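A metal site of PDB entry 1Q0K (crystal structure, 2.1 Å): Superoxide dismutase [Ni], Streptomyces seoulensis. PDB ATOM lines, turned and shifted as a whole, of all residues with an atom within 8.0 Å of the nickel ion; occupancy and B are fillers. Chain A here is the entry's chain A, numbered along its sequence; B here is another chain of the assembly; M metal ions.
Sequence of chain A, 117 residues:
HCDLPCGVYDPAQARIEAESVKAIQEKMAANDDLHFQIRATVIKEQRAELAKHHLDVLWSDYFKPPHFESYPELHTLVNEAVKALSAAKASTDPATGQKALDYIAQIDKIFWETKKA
A ring nitrogen (ND1) of His 1 lies within hydrogen-bond range of the backbone carbonyl oxygen of Val 8.
N of Val 8 sits close to SG of Cys 6 (3.2 Å).
The guanidinium group (NH2) of Arg 47 of chain B lies within hydrogen-bond range of a ring nitrogen (NE2) of His 1, at 3.2 Å.
The side-chain carboxylate of Glu 17 of chain B lies within hydrogen-bond range of a ring nitrogen (NE2) of His 1 (3.1 Å).
OG of Ser 20 of chain B sits close to SG of Cys 6, at 3.4 Å.
Residues that only touch the nickel ion: Asp 3 (3.7 Å).
Within 4 Å of the nickel ion: His 1, Cys 2, Asp 3 and Cys 6.
The nearest printed residue that does not touch the nickel ion is Val 8 (4.2 Å).
The nickel ion is bound by N of Cys 2 (2.0 Å), N of His 1 (2.2 Å), SG of Cys 6 (2.3 Å) and SG of Cys 2 (2.3 Å).
The nickel ion has four donor atoms within binding distance.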
ATOM      1  N   HIS A   1       2.449 -14.713  13.888  1.00  0.00           N
ATOM      2  CA  HIS A   1       2.164 -16.139  13.572  1.00  0.00           C
ATOM      3  C   HIS A   1       2.436 -17.048  14.769  1.00  0.00           C
ATOM      4  O   HIS A   1       2.176 -18.249  14.727  1.00  0.00           O
ATOM      5  CB  HIS A   1       3.020 -16.599  12.396  1.00  0.00           C
ATOM      6  CG  HIS A   1       4.491 -16.498  12.638  1.00  0.00           C
ATOM      7  ND1 HIS A   1       5.196 -15.328  12.508  1.00  0.00           N
ATOM      8  CD2 HIS A   1       5.403 -17.440  13.014  1.00  0.00           C
ATOM      9  CE1 HIS A   1       6.470 -15.535  12.796  1.00  0.00           C
ATOM     10  NE2 HIS A   1       6.620 -16.815  13.102  1.00  0.00           N
ATOM     11  N   CYS A   2       2.967 -16.468  15.841  1.00  0.00           N
ATOM     12  CA  CYS A   2       3.300 -17.205  17.049  1.00  0.00           C
ATOM     13  C   CYS A   2       2.164 -17.192  18.071  1.00  0.00           C
ATOM     14  O   CYS A   2       2.259 -17.838  19.132  1.00  0.00           O
ATOM     15  CB  CYS A   2       4.549 -16.588  17.674  1.00  0.00           C
ATOM     16  SG  CYS A   2       4.373 -14.811  17.903  1.00  0.00           S
ATOM     17  N   ASP A   3       1.101 -16.459  17.755  1.00  0.00           N
ATOM     18  CA  ASP A   3      -0.096 -16.351  18.596  1.00  0.00           C
ATOM     19  C   ASP A   3       0.040 -15.516  19.873  1.00  0.00           C
ATOM     20  O   ASP A   3      -0.812 -15.614  20.770  1.00  0.00           O
ATOM     21  CB  ASP A   3      -0.614 -17.753  18.954  1.00  0.00           C
ATOM     22  CG  ASP A   3      -2.124 -17.794  19.061  1.00  0.00           C
ATOM     23  OD1 ASP A   3      -2.766 -16.755  18.827  1.00  0.00           O
ATOM     24  OD2 ASP A   3      -2.669 -18.871  19.390  1.00  0.00           O
ATOM     25  N   LEU A   4       1.086 -14.696  19.979  1.00  0.00           N
ATOM     26  CA  LEU A   4       1.259 -13.840  21.161  1.00  0.00           C
ATOM     27  C   LEU A   4       0.072 -12.885  21.313  1.00  0.00           C
ATOM     28  O   LEU A   4      -0.480 -12.744  22.395  1.00  0.00           O
ATOM     29  CB  LEU A   4       2.545 -13.008  21.076  1.00  0.00           C
ATOM     30  CG  LEU A   4       2.645 -11.897  22.138  1.00  0.00           C
ATOM     31  CD1 LEU A   4       2.669 -12.523  23.524  1.00  0.00           C
ATOM     32  CD2 LEU A   4       3.878 -11.057  21.919  1.00  0.00           C
ATOM     33  N   PRO A   5      -0.328 -12.212  20.214  1.00  0.00           N
ATOM     34  CA  PRO A   5       0.229 -12.280  18.857  1.00  0.00           C
ATOM     35  C   PRO A   5       1.432 -11.357  18.681  1.00  0.00           C
ATOM     36  O   PRO A   5       1.654 -10.452  19.484  1.00  0.00           O
ATOM     37  CB  PRO A   5      -0.950 -11.864  17.988  1.00  0.00           C
ATOM     38  CG  PRO A   5      -1.592 -10.803  18.826  1.00  0.00           C
ATOM     39  CD  PRO A   5      -1.580 -11.423  20.216  1.00  0.00           C
ATOM     40  N   CYS A   6       2.201 -11.587  17.631  1.00  0.00           N
ATOM     41  CA  CYS A   6       3.388 -10.786  17.370  1.00  0.00           C
ATOM     42  C   CYS A   6       3.163  -9.806  16.213  1.00  0.00           C
ATOM     43  O   CYS A   6       3.918  -8.839  16.055  1.00  0.00           O
ATOM     44  CB  CYS A   6       4.571 -11.687  17.044  1.00  0.00           C
ATOM     45  SG  CYS A   6       4.397 -12.510  15.446  1.00  0.00           S
ATOM     46  N   GLY A   7       2.143 -10.070  15.413  1.00  0.00           N
ATOM     47  CA  GLY A   7       1.829  -9.213  14.279  1.00  0.00           C
ATOM     48  C   GLY A   7       2.653  -9.490  13.027  1.00  0.00           C
ATOM     49  O   GLY A   7       2.546  -8.759  12.035  1.00  0.00           O
ATOM     50  N   VAL A   8       3.470 -10.546  13.060  1.00  0.00           N
ATOM     51  CA  VAL A   8       4.321 -10.890  11.922  1.00  0.00           C
ATOM     52  C   VAL A   8       3.792 -12.133  11.197  1.00  0.00           C
ATOM     53  O   VAL A   8       3.775 -13.227  11.762  1.00  0.00           O
ATOM     54  CB  VAL A   8       5.784 -11.140  12.378  1.00  0.00           C
ATOM     55  CG1 VAL A   8       6.685 -11.410  11.164  1.00  0.00           C
ATOM     56  CG2 VAL A   8       6.299  -9.945  13.171  1.00  0.00           C
ATOM     57  N   TYR A   9       3.383 -11.967   9.941  1.00  0.00           N
ATOM     58  CA  TYR A   9       2.867 -13.074   9.146  1.00  0.00           C
ATOM     59  C   TYR A   9       3.334 -12.966   7.703  1.00  0.00           C
ATOM     60  O   TYR A   9       3.590 -11.867   7.202  1.00  0.00           O
ATOM     61  CB  TYR A   9       1.328 -13.074   9.127  1.00  0.00           C
ATOM     62  CG  TYR A   9       0.651 -13.182  10.461  1.00  0.00           C
ATOM     63  CD1 TYR A   9       0.332 -12.034  11.199  1.00  0.00           C
ATOM     64  CD2 TYR A   9       0.272 -14.416  10.985  1.00  0.00           C
ATOM     65  CE1 TYR A   9      -0.342 -12.120  12.407  1.00  0.00           C
ATOM     66  CE2 TYR A   9      -0.406 -14.514  12.201  1.00  0.00           C
ATOM     67  CZ  TYR A   9      -0.702 -13.351  12.906  1.00  0.00           C
ATOM     68  OH  TYR A   9      -1.376 -13.417  14.106  1.00  0.00           O
ATOM     69  N   GLN A  13       6.073 -18.454   4.151  1.00  0.00           N
ATOM     70  CA  GLN A  13       6.485 -19.595   4.963  1.00  0.00           C
ATOM     71  C   GLN A  13       5.869 -20.859   4.388  1.00  0.00           C
ATOM     72  O   GLN A  13       6.543 -21.886   4.258  1.00  0.00           O
ATOM     73  CB  GLN A  13       6.051 -19.422   6.423  1.00  0.00           C
ATOM     74  CG  GLN A  13       6.744 -18.263   7.148  1.00  0.00           C
ATOM     75  CD  GLN A  13       6.472 -18.254   8.658  1.00  0.00           C
ATOM     76  OE1 GLN A  13       5.356 -17.975   9.107  1.00  0.00           O
ATOM     77  NE2 GLN A  13       7.500 -18.585   9.443  1.00  0.00           N
ATOM     78  N   VAL A  57      -2.411 -21.449  10.364  1.00  0.00           N
ATOM     79  CA  VAL A  57      -2.173 -20.292  11.233  1.00  0.00           C
ATOM     80  C   VAL A  57      -2.663 -19.009  10.594  1.00  0.00           C
ATOM     81  O   VAL A  57      -3.210 -18.155  11.290  1.00  0.00           O
ATOM     82  CB  VAL A  57      -0.658 -20.141  11.589  1.00  0.00           C
ATOM     83  CG1 VAL A  57      -0.404 -18.794  12.261  1.00  0.00           C
ATOM     84  CG2 VAL A  57      -0.227 -21.271  12.535  1.00  0.00           C
ATOM     85  N   ASP A  61      -5.211 -17.398  12.901  1.00  0.00           N
ATOM     86  CA  ASP A  61      -4.673 -16.227  13.577  1.00  0.00           C
ATOM     87  C   ASP A  61      -4.671 -14.910  12.821  1.00  0.00           C
ATOM     88  O   ASP A  61      -4.986 -13.867  13.403  1.00  0.00           O
ATOM     89  CB  ASP A  61      -3.248 -16.543  14.060  1.00  0.00           C
ATOM     90  CG  ASP A  61      -3.207 -17.658  15.090  1.00  0.00           C
ATOM     91  OD1 ASP A  61      -4.194 -18.420  15.223  1.00  0.00           O
ATOM     92  OD2 ASP A  61      -2.171 -17.783  15.777  1.00  0.00           O
ATOM     93  N   ILE B  16      12.066 -13.876   9.078  1.00  0.00           N
ATOM     94  CA  ILE B  16      10.700 -13.705   9.579  1.00  0.00           C
ATOM     95  C   ILE B  16      10.629 -14.056  11.064  1.00  0.00           C
ATOM     96  O   ILE B  16       9.940 -13.381  11.827  1.00  0.00           O
ATOM     97  CB  ILE B  16       9.705 -14.595   8.794  1.00  0.00           C
ATOM     98  CG1 ILE B  16       9.795 -14.262   7.293  1.00  0.00           C
ATOM     99  CG2 ILE B  16       8.288 -14.340   9.277  1.00  0.00           C
ATOM    100  CD1 ILE B  16       9.021 -15.213   6.386  1.00  0.00           C
ATOM    101  N   GLU B  17      11.355 -15.083  11.467  1.00  0.00           N
ATOM    102  CA  GLU B  17      11.368 -15.501  12.867  1.00  0.00           C
ATOM    103  C   GLU B  17      12.080 -14.444  13.714  1.00  0.00           C
ATOM    104  O   GLU B  17      11.647 -14.147  14.829  1.00  0.00           O
ATOM    105  CB  GLU B  17      12.070 -16.849  13.027  1.00  0.00           C
ATOM    106  CG  GLU B  17      11.317 -18.008  12.376  1.00  0.00           C
ATOM    107  CD  GLU B  17       9.887 -18.128  12.885  1.00  0.00           C
ATOM    108  OE1 GLU B  17       9.520 -17.422  13.851  1.00  0.00           O
ATOM    109  OE2 GLU B  17       9.110 -18.940  12.320  1.00  0.00           O
ATOM    110  N   SER B  20       9.792 -11.428  14.374  1.00  0.00           N
ATOM    111  CA  SER B  20       8.834 -11.591  15.466  1.00  0.00           C
ATOM    112  C   SER B  20       9.538 -11.268  16.773  1.00  0.00           C
ATOM    113  O   SER B  20       8.960 -10.635  17.651  1.00  0.00           O
ATOM    114  CB  SER B  20       8.301 -13.035  15.513  1.00  0.00           C
ATOM    115  OG  SER B  20       7.541 -13.342  14.359  1.00  0.00           O
ATOM    116  N   VAL B  21      10.794 -11.701  16.898  1.00  0.00           N
ATOM    117  CA  VAL B  21      11.565 -11.455  18.111  1.00  0.00           C
ATOM    118  C   VAL B  21      11.624  -9.976  18.454  1.00  0.00           C
ATOM    119  O   VAL B  21      11.345  -9.596  19.600  1.00  0.00           O
ATOM    120  CB  VAL B  21      13.026 -11.969  17.981  1.00  0.00           C
ATOM    121  CG1 VAL B  21      13.853 -11.515  19.179  1.00  0.00           C
ATOM    122  CG2 VAL B  21      13.035 -13.483  17.888  1.00  0.00           C
ATOM    123  N   ALA B  23       9.703  -7.564  17.210  1.00  0.00           N
ATOM    124  CA  ALA B  23       8.340  -7.083  17.356  1.00  0.00           C
ATOM    125  C   ALA B  23       7.827  -7.371  18.770  1.00  0.00           C
ATOM    126  O   ALA B  23       7.192  -6.522  19.397  1.00  0.00           O
ATOM    127  CB  ALA B  23       7.425  -7.752  16.334  1.00  0.00           C
ATOM    128  N   ILE B  24       8.124  -8.563  19.273  1.00  0.00           N
ATOM    129  CA  ILE B  24       7.712  -8.942  20.616  1.00  0.00           C
ATOM    130  C   ILE B  24       8.419  -8.083  21.656  1.00  0.00           C
ATOM    131  O   ILE B  24       7.800  -7.630  22.614  1.00  0.00           O
ATOM    132  CB  ILE B  24       8.006 -10.434  20.878  1.00  0.00           C
ATOM    133  CG1 ILE B  24       7.119 -11.298  19.990  1.00  0.00           C
ATOM    134  CG2 ILE B  24       7.796 -10.769  22.354  1.00  0.00           C
ATOM    135  CD1 ILE B  24       7.521 -12.764  19.960  1.00  0.00           C
ATOM    136  N   ILE B  43       7.130 -16.953  24.095  1.00  0.00           N
ATOM    137  CA  ILE B  43       7.043 -16.939  22.645  1.00  0.00           C
ATOM    138  C   ILE B  43       8.281 -16.370  21.966  1.00  0.00           C
ATOM    139  O   ILE B  43       8.652 -16.800  20.874  1.00  0.00           O
ATOM    140  CB  ILE B  43       5.790 -16.169  22.192  1.00  0.00           C
ATOM    141  CG1 ILE B  43       4.544 -16.876  22.737  1.00  0.00           C
ATOM    142  CG2 ILE B  43       5.741 -16.095  20.679  1.00  0.00           C
ATOM    143  CD1 ILE B  43       3.238 -16.275  22.267  1.00  0.00           C
ATOM    144  N   ARG B  47      10.577 -18.229  19.020  1.00  0.00           N
ATOM    145  CA  ARG B  47      10.872 -17.614  17.732  1.00  0.00           C
ATOM    146  C   ARG B  47      12.370 -17.441  17.472  1.00  0.00           C
ATOM    147  O   ARG B  47      12.830 -17.620  16.338  1.00  0.00           O
ATOM    148  CB  ARG B  47      10.178 -16.245  17.608  1.00  0.00           C
ATOM    149  CG  ARG B  47       8.712 -16.215  18.058  1.00  0.00           C
ATOM    150  CD  ARG B  47       7.981 -17.542  17.885  1.00  0.00           C
ATOM    151  NE  ARG B  47       7.869 -17.958  16.493  1.00  0.00           N
ATOM    152  CZ  ARG B  47       7.310 -19.099  16.092  1.00  0.00           C
ATOM    153  NH1 ARG B  47       6.801 -19.945  16.988  1.00  0.00           N
ATOM    154  NH2 ARG B  47       7.249 -19.407  14.810  1.00  0.00           N
HETATM  155 NI    NI M   1       3.529 -14.576  15.765  1.00  0.00          NI
